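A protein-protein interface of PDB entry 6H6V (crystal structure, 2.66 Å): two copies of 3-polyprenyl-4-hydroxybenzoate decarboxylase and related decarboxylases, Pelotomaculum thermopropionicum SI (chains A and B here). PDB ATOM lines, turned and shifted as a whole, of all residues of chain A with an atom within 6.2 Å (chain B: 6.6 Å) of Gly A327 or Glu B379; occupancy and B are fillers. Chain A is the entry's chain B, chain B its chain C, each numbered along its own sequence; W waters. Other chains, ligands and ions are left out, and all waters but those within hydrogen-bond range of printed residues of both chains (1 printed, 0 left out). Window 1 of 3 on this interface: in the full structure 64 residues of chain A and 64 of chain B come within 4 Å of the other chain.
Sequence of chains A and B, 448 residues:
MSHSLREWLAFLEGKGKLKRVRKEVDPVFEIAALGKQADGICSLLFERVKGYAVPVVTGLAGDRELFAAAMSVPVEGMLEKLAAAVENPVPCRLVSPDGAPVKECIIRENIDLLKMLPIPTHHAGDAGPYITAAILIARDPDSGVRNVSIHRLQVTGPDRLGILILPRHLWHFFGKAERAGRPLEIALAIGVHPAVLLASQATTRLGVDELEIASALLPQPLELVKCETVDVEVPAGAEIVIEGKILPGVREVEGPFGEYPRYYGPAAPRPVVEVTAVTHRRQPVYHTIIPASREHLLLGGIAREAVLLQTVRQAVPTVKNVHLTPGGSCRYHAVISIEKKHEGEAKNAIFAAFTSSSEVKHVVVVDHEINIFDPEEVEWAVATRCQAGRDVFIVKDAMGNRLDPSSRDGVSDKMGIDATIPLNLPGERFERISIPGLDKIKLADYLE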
ATOM      1  N   ARG A 262      -7.171  -6.559 -26.076  1.00  0.00           N
ATOM      2  CA  ARG A 262      -5.900  -6.947 -26.656  1.00  0.00           C
ATOM      3  C   ARG A 262      -5.211  -8.069 -25.847  1.00  0.00           C
ATOM      4  O   ARG A 262      -4.010  -8.157 -25.830  1.00  0.00           O
ATOM      5  CB  ARG A 262      -4.999  -5.695 -26.917  1.00  0.00           C
ATOM      6  CG  ARG A 262      -5.519  -4.787 -28.042  1.00  0.00           C
ATOM      7  CD  ARG A 262      -5.061  -3.321 -28.019  1.00  0.00           C
ATOM      8  NE  ARG A 262      -6.205  -2.420 -28.317  1.00  0.00           N
ATOM      9  CZ  ARG A 262      -6.280  -1.099 -28.015  1.00  0.00           C
ATOM     10  NH1 ARG A 262      -5.267  -0.437 -27.416  1.00  0.00           N
ATOM     11  NH2 ARG A 262      -7.389  -0.413 -28.320  1.00  0.00           N
ATOM     12  N   ARG A 294     -11.764  -0.324 -33.576  1.00  0.00           N
ATOM     13  CA  ARG A 294     -12.584   0.780 -33.133  1.00  0.00           C
ATOM     14  C   ARG A 294     -14.069   0.463 -33.283  1.00  0.00           C
ATOM     15  O   ARG A 294     -14.875   0.845 -32.430  1.00  0.00           O
ATOM     16  CB  ARG A 294     -12.224   2.017 -33.948  1.00  0.00           C
ATOM     17  CG  ARG A 294     -11.864   3.212 -33.137  1.00  0.00           C
ATOM     18  CD  ARG A 294     -10.632   2.987 -32.280  1.00  0.00           C
ATOM     19  NE  ARG A 294     -10.180   4.304 -31.887  1.00  0.00           N
ATOM     20  CZ  ARG A 294      -9.036   4.542 -31.252  1.00  0.00           C
ATOM     21  NH1 ARG A 294      -8.202   3.538 -30.937  1.00  0.00           N
ATOM     22  NH2 ARG A 294      -8.710   5.804 -30.995  1.00  0.00           N
ATOM     23  N   THR A 325     -12.643   5.626 -22.674  1.00  0.00           N
ATOM     24  CA  THR A 325     -11.537   5.878 -23.603  1.00  0.00           C
ATOM     25  C   THR A 325     -11.137   4.604 -24.318  1.00  0.00           C
ATOM     26  O   THR A 325     -11.246   3.520 -23.763  1.00  0.00           O
ATOM     27  CB  THR A 325     -10.292   6.472 -22.905  1.00  0.00           C
ATOM     28  OG1 THR A 325      -9.728   5.496 -22.028  1.00  0.00           O
ATOM     29  CG2 THR A 325     -10.626   7.710 -22.098  1.00  0.00           C
ATOM     30  N   PRO A 326     -10.662   4.734 -25.561  1.00  0.00           N
ATOM     31  CA  PRO A 326     -10.158   3.560 -26.285  1.00  0.00           C
ATOM     32  C   PRO A 326      -8.918   2.933 -25.638  1.00  0.00           C
ATOM     33  O   PRO A 326      -8.687   1.711 -25.782  1.00  0.00           O
ATOM     34  CB  PRO A 326      -9.856   4.094 -27.674  1.00  0.00           C
ATOM     35  CG  PRO A 326      -9.809   5.564 -27.547  1.00  0.00           C
ATOM     36  CD  PRO A 326     -10.652   5.954 -26.392  1.00  0.00           C
ATOM     37  N   GLY A 327      -8.145   3.745 -24.926  1.00  0.00           N
ATOM     38  CA  GLY A 327      -7.039   3.248 -24.127  1.00  0.00           C
ATOM     39  C   GLY A 327      -7.489   2.239 -23.079  1.00  0.00           C
ATOM     40  O   GLY A 327      -6.781   1.295 -22.793  1.00  0.00           O
ATOM     41  N   GLY A 328      -8.675   2.442 -22.520  1.00  0.00           N
ATOM     42  CA  GLY A 328      -9.278   1.472 -21.606  1.00  0.00           C
ATOM     43  C   GLY A 328     -10.209   0.439 -22.223  1.00  0.00           C
ATOM     44  O   GLY A 328     -11.029  -0.130 -21.516  1.00  0.00           O
ATOM     45  N   SER A 329     -10.070   0.196 -23.523  1.00  0.00           N
ATOM     46  CA  SER A 329     -10.995  -0.661 -24.288  1.00  0.00           C
ATOM     47  C   SER A 329     -12.473  -0.237 -24.179  1.00  0.00           C
ATOM     48  O   SER A 329     -13.372  -1.083 -24.196  1.00  0.00           O
ATOM     49  CB  SER A 329     -10.806  -2.130 -23.879  1.00  0.00           C
ATOM     50  OG  SER A 329      -9.433  -2.455 -23.798  1.00  0.00           O
ATOM     51  N   CYS A 330     -12.707   1.065 -24.092  1.00  0.00           N
ATOM     52  CA  CYS A 330     -14.058   1.634 -24.009  1.00  0.00           C
ATOM     53  C   CYS A 330     -14.903   0.907 -22.961  1.00  0.00           C
ATOM     54  O   CYS A 330     -15.979   0.416 -23.239  1.00  0.00           O
ATOM     55  CB  CYS A 330     -14.712   1.634 -25.398  1.00  0.00           C
ATOM     56  SG  CYS A 330     -13.785   2.656 -26.604  1.00  0.00           S
ATOM     57  N   TYR A 332     -12.908   0.358 -19.278  1.00  0.00           N
ATOM     58  CA  TYR A 332     -12.139   0.330 -18.053  1.00  0.00           C
ATOM     59  C   TYR A 332     -11.809   1.726 -17.534  1.00  0.00           C
ATOM     60  O   TYR A 332     -11.758   1.930 -16.336  1.00  0.00           O
ATOM     61  CB  TYR A 332     -10.815  -0.423 -18.255  1.00  0.00           C
ATOM     62  CG  TYR A 332     -10.896  -1.883 -18.630  1.00  0.00           C
ATOM     63  CD1 TYR A 332     -11.775  -2.753 -17.992  1.00  0.00           C
ATOM     64  CD2 TYR A 332     -10.031  -2.416 -19.573  1.00  0.00           C
ATOM     65  CE1 TYR A 332     -11.820  -4.106 -18.317  1.00  0.00           C
ATOM     66  CE2 TYR A 332     -10.071  -3.765 -19.919  1.00  0.00           C
ATOM     67  CZ  TYR A 332     -10.951  -4.606 -19.266  1.00  0.00           C
ATOM     68  OH  TYR A 332     -10.989  -5.931 -19.593  1.00  0.00           O
ATOM     69  N   HIS A 333     -11.534   2.651 -18.433  1.00  0.00           N
ATOM     70  CA  HIS A 333     -11.205   4.031 -18.075  1.00  0.00           C
ATOM     71  C   HIS A 333     -12.347   4.951 -18.459  1.00  0.00           C
ATOM     72  O   HIS A 333     -12.844   4.897 -19.582  1.00  0.00           O
ATOM     73  CB  HIS A 333      -9.943   4.467 -18.824  1.00  0.00           C
ATOM     74  CG  HIS A 333      -8.692   3.864 -18.280  1.00  0.00           C
ATOM     75  ND1 HIS A 333      -7.453   4.174 -18.790  1.00  0.00           N
ATOM     76  CD2 HIS A 333      -8.483   3.006 -17.247  1.00  0.00           C
ATOM     77  CE1 HIS A 333      -6.533   3.507 -18.103  1.00  0.00           C
ATOM     78  NE2 HIS A 333      -7.130   2.793 -17.159  1.00  0.00           N
ATOM     79  N   VAL A 335     -13.639   9.123 -18.317  1.00  0.00           N
ATOM     80  CA  VAL A 335     -13.344  10.515 -18.065  1.00  0.00           C
ATOM     81  C   VAL A 335     -14.653  11.255 -18.042  1.00  0.00           C
ATOM     82  O   VAL A 335     -15.427  11.178 -19.000  1.00  0.00           O
ATOM     83  CB  VAL A 335     -12.468  11.082 -19.169  1.00  0.00           C
ATOM     84  CG1 VAL A 335     -12.115  12.552 -18.867  1.00  0.00           C
ATOM     85  CG2 VAL A 335     -11.211  10.209 -19.342  1.00  0.00           C
ATOM     86  N   PRO A 375      -6.895  13.142 -25.284  1.00  0.00           N
ATOM     87  CA  PRO A 375      -6.129  12.567 -24.153  1.00  0.00           C
ATOM     88  C   PRO A 375      -5.093  13.512 -23.565  1.00  0.00           C
ATOM     89  O   PRO A 375      -4.924  13.559 -22.351  1.00  0.00           O
ATOM     90  CB  PRO A 375      -5.447  11.336 -24.750  1.00  0.00           C
ATOM     91  CG  PRO A 375      -6.183  11.039 -25.998  1.00  0.00           C
ATOM     92  CD  PRO A 375      -6.777  12.331 -26.501  1.00  0.00           C
ATOM     93  N   ASP B 374       3.628   6.431 -27.413  1.00  0.00           N
ATOM     94  CA  ASP B 374       2.215   6.319 -27.780  1.00  0.00           C
ATOM     95  C   ASP B 374       1.354   6.361 -26.507  1.00  0.00           C
ATOM     96  O   ASP B 374       1.308   5.375 -25.764  1.00  0.00           O
ATOM     97  CB  ASP B 374       1.951   5.003 -28.523  1.00  0.00           C
ATOM     98  CG  ASP B 374       0.521   4.890 -29.069  1.00  0.00           C
ATOM     99  OD1 ASP B 374      -0.378   5.696 -28.700  1.00  0.00           O
ATOM    100  OD2 ASP B 374       0.294   3.976 -29.879  1.00  0.00           O
ATOM    101  N   PRO B 375       0.646   7.483 -26.267  1.00  0.00           N
ATOM    102  CA  PRO B 375      -0.139   7.610 -25.022  1.00  0.00           C
ATOM    103  C   PRO B 375      -1.176   6.516 -24.836  1.00  0.00           C
ATOM    104  O   PRO B 375      -1.365   6.032 -23.724  1.00  0.00           O
ATOM    105  CB  PRO B 375      -0.828   8.973 -25.150  1.00  0.00           C
ATOM    106  CG  PRO B 375      -0.076   9.703 -26.194  1.00  0.00           C
ATOM    107  CD  PRO B 375       0.546   8.680 -27.110  1.00  0.00           C
ATOM    108  N   GLU B 376      -1.824   6.127 -25.922  1.00  0.00           N
ATOM    109  CA  GLU B 376      -2.811   5.063 -25.872  1.00  0.00           C
ATOM    110  C   GLU B 376      -2.228   3.722 -25.422  1.00  0.00           C
ATOM    111  O   GLU B 376      -2.871   2.993 -24.681  1.00  0.00           O
ATOM    112  CB  GLU B 376      -3.494   4.900 -27.223  1.00  0.00           C
ATOM    113  CG  GLU B 376      -4.736   4.050 -27.120  1.00  0.00           C
ATOM    114  CD  GLU B 376      -5.476   3.870 -28.418  1.00  0.00           C
ATOM    115  OE1 GLU B 376      -5.782   4.907 -29.067  1.00  0.00           O
ATOM    116  OE2 GLU B 376      -5.779   2.684 -28.742  1.00  0.00           O
ATOM    117  N   GLU B 377      -1.015   3.399 -25.857  1.00  0.00           N
ATOM    118  CA  GLU B 377      -0.403   2.133 -25.479  1.00  0.00           C
ATOM    119  C   GLU B 377      -0.041   2.129 -23.981  1.00  0.00           C
ATOM    120  O   GLU B 377      -0.208   1.107 -23.313  1.00  0.00           O
ATOM    121  CB  GLU B 377       0.802   1.835 -26.358  1.00  0.00           C
ATOM    122  CG  GLU B 377       1.034   0.337 -26.576  1.00  0.00           C
ATOM    123  CD  GLU B 377       2.043   0.035 -27.691  1.00  0.00           C
ATOM    124  OE1 GLU B 377       1.760   0.384 -28.858  1.00  0.00           O
ATOM    125  OE2 GLU B 377       3.106  -0.561 -27.402  1.00  0.00           O
ATOM    126  N   VAL B 378       0.381   3.271 -23.424  1.00  0.00           N
ATOM    127  CA  VAL B 378       0.710   3.281 -21.999  1.00  0.00           C
ATOM    128  C   VAL B 378      -0.570   3.288 -21.177  1.00  0.00           C
ATOM    129  O   VAL B 378      -0.632   2.611 -20.150  1.00  0.00           O
ATOM    130  CB  VAL B 378       1.766   4.341 -21.528  1.00  0.00           C
ATOM    131  CG1 VAL B 378       2.584   4.914 -22.672  1.00  0.00           C
ATOM    132  CG2 VAL B 378       1.178   5.449 -20.673  1.00  0.00           C
ATOM    133  N   GLU B 379      -1.593   4.028 -21.624  1.00  0.00           N
ATOM    134  CA  GLU B 379      -2.901   4.002 -20.959  1.00  0.00           C
ATOM    135  C   GLU B 379      -3.473   2.579 -20.925  1.00  0.00           C
ATOM    136  O   GLU B 379      -4.040   2.149 -19.921  1.00  0.00           O
ATOM    137  CB  GLU B 379      -3.900   4.946 -21.645  1.00  0.00           C
ATOM    138  CG  GLU B 379      -5.182   5.117 -20.852  1.00  0.00           C
ATOM    139  CD  GLU B 379      -6.326   5.805 -21.585  1.00  0.00           C
ATOM    140  OE1 GLU B 379      -7.486   5.718 -21.068  1.00  0.00           O
ATOM    141  OE2 GLU B 379      -6.076   6.413 -22.662  1.00  0.00           O
ATOM    142  N   TRP B 380      -3.321   1.863 -22.037  1.00  0.00           N
ATOM    143  CA  TRP B 380      -3.711   0.472 -22.121  1.00  0.00           C
ATOM    144  C   TRP B 380      -2.999  -0.376 -21.078  1.00  0.00           C
ATOM    145  O   TRP B 380      -3.627  -1.168 -20.361  1.00  0.00           O
ATOM    146  CB  TRP B 380      -3.427  -0.051 -23.528  1.00  0.00           C
ATOM    147  CG  TRP B 380      -3.671  -1.483 -23.651  1.00  0.00           C
ATOM    148  CD1 TRP B 380      -4.874  -2.091 -23.786  1.00  0.00           C
ATOM    149  CD2 TRP B 380      -2.696  -2.510 -23.617  1.00  0.00           C
ATOM    150  NE1 TRP B 380      -4.706  -3.452 -23.858  1.00  0.00           N
ATOM    151  CE2 TRP B 380      -3.376  -3.736 -23.768  1.00  0.00           C
ATOM    152  CE3 TRP B 380      -1.313  -2.519 -23.489  1.00  0.00           C
ATOM    153  CZ2 TRP B 380      -2.731  -4.955 -23.783  1.00  0.00           C
ATOM    154  CZ3 TRP B 380      -0.650  -3.741 -23.571  1.00  0.00           C
ATOM    155  CH2 TRP B 380      -1.367  -4.949 -23.710  1.00  0.00           C
ATOM    156  N   ALA B 381      -1.693  -0.199 -20.992  1.00  0.00           N
ATOM    157  CA  ALA B 381      -0.903  -0.896 -19.981  1.00  0.00           C
ATOM    158  C   ALA B 381      -1.397  -0.587 -18.559  1.00  0.00           C
ATOM    159  O   ALA B 381      -1.537  -1.501 -17.746  1.00  0.00           O
ATOM    160  CB  ALA B 381       0.580  -0.545 -20.125  1.00  0.00           C
ATOM    161  N   VAL B 382      -1.688   0.685 -18.273  1.00  0.00           N
ATOM    162  CA  VAL B 382      -2.226   1.053 -16.971  1.00  0.00           C
ATOM    163  C   VAL B 382      -3.589   0.406 -16.730  1.00  0.00           C
ATOM    164  O   VAL B 382      -3.867  -0.069 -15.634  1.00  0.00           O
ATOM    165  CB  VAL B 382      -2.335   2.594 -16.810  1.00  0.00           C
ATOM    166  CG1 VAL B 382      -3.007   2.961 -15.491  1.00  0.00           C
ATOM    167  CG2 VAL B 382      -0.958   3.239 -16.844  1.00  0.00           C
ATOM    168  N   ALA B 383      -4.437   0.377 -17.742  1.00  0.00           N
ATOM    169  CA  ALA B 383      -5.781  -0.178 -17.576  1.00  0.00           C
ATOM    170  C   ALA B 383      -5.759  -1.669 -17.253  1.00  0.00           C
ATOM    171  O   ALA B 383      -6.615  -2.149 -16.504  1.00  0.00           O
ATOM    172  CB  ALA B 383      -6.610   0.047 -18.826  1.00  0.00           C
ATOM    173  N   THR B 384      -4.797  -2.395 -17.812  1.00  0.00           N
ATOM    174  CA  THR B 384      -4.829  -3.843 -17.749  1.00  0.00           C
ATOM    175  C   THR B 384      -3.715  -4.489 -16.959  1.00  0.00           C
ATOM    176  O   THR B 384      -3.752  -5.702 -16.767  1.00  0.00           O
ATOM    177  CB  THR B 384      -4.771  -4.425 -19.159  1.00  0.00           C
ATOM    178  OG1 THR B 384      -3.557  -4.020 -19.793  1.00  0.00           O
ATOM    179  CG2 THR B 384      -5.962  -3.937 -19.974  1.00  0.00           C
HETATM  180  O   HOH W   1      -7.616   6.359 -24.991  1.00  0.00           O
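The side-chain hydroxyl of Thr A325 is in hydrogen-bond range of the side-chain carboxylate of Glu B379 (2.4 Å).
The side-chain carboxylate of Glu B376 is in salt-bridge range of the guanidinium group of Arg A262 (3.4 Å).
The side-chain carboxylate (OE1) of Glu B379 sits at hydrogen-bond distance from a ring nitrogen (ND1) of His A333 (2.8 Å).
The side-chain carboxylate of Glu B376 is in salt-bridge range of the guanidinium group of Arg A294 (3.4 Å).
Position printed for both chains: 375.
Of the 10 pairs that touch across the chains among the printed residues, none has its exchanged pair printed and touching as well.
Among the printed residues, merely in contact across the chains: Arg A262 with Trp B380 (3.8 Å), Gly A327 with Glu B376 (3.9 Å), Gly A327 with Glu B379 (3.6 Å), Gly A327 with Trp B380 (3.2 Å), Gly A328 with Glu B379 (3.8 Å) and His A333 with Ala B383 (3.3 Å).
O of Trp B380 sits at hydrogen-bond distance from OG1 of Thr B384 (2.9 Å).
The side-chain carboxylate (OD1) of Asp B374 is in hydrogen-bond range of the backbone NH (N) of Glu B376.
O of Thr A325 sits at hydrogen-bond distance from N of Cys A330, 2.9 Å away.
The side-chain hydroxyl (OG1) of Thr A325 lies within hydrogen-bond range of the backbone NH (N) of Gly A328 (3.3 Å).
O of His A333 sits at hydrogen-bond distance from N of Thr A325 (3.2 Å).
Of chain B, only Glu B376 (3.9 Å), Glu B379 (3.6 Å) and Trp B380 (3.2 Å) come within 4 Å of Gly A327.
Of the printed residues of chain B, Arg A294 touches Glu B376 (3.4 Å).
Of the printed residues of chain B, Gly A328 touches Glu B379 (3.8 Å).
Printed residues of chain A within 4 Å of Glu B376: Arg A262 (3.4 Å), Arg A294 (3.4 Å) and Gly A327 (3.9 Å).
Printed residues of chain A within 4 Å of Trp B380: Arg A262 (3.8 Å) and Gly A327 (3.2 Å).
Printed residues of chain B within 4 Å of Thr A325: Glu B379 (2.4 Å).
Cys A330 touches none of the printed residues of chain B.
The nearest printed residue of chain A that does not touch Glu B379 is Pro A375 (5.4 Å).
The nearest printed residue of chain B that does not touch Gly A328 is Ala B383 (4.1 Å).
Hydrophobic or aromatic side chains of chain B within 4 Å of the printed part of chain A: Trp B380 and Ala B383.
Along chain B the printed residues that touch a printed residue of chain A span positions 376 to 383.
Of the 12 printed residues of chain A, 6 touch a printed residue of chain B.
Among the printed residues, 10 pairs touch across the chains.
Water W1 bridges the backbone NH of Gly A327 (2.7 Å) and the side-chain carboxylate of Glu B379 (2.8 Å).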
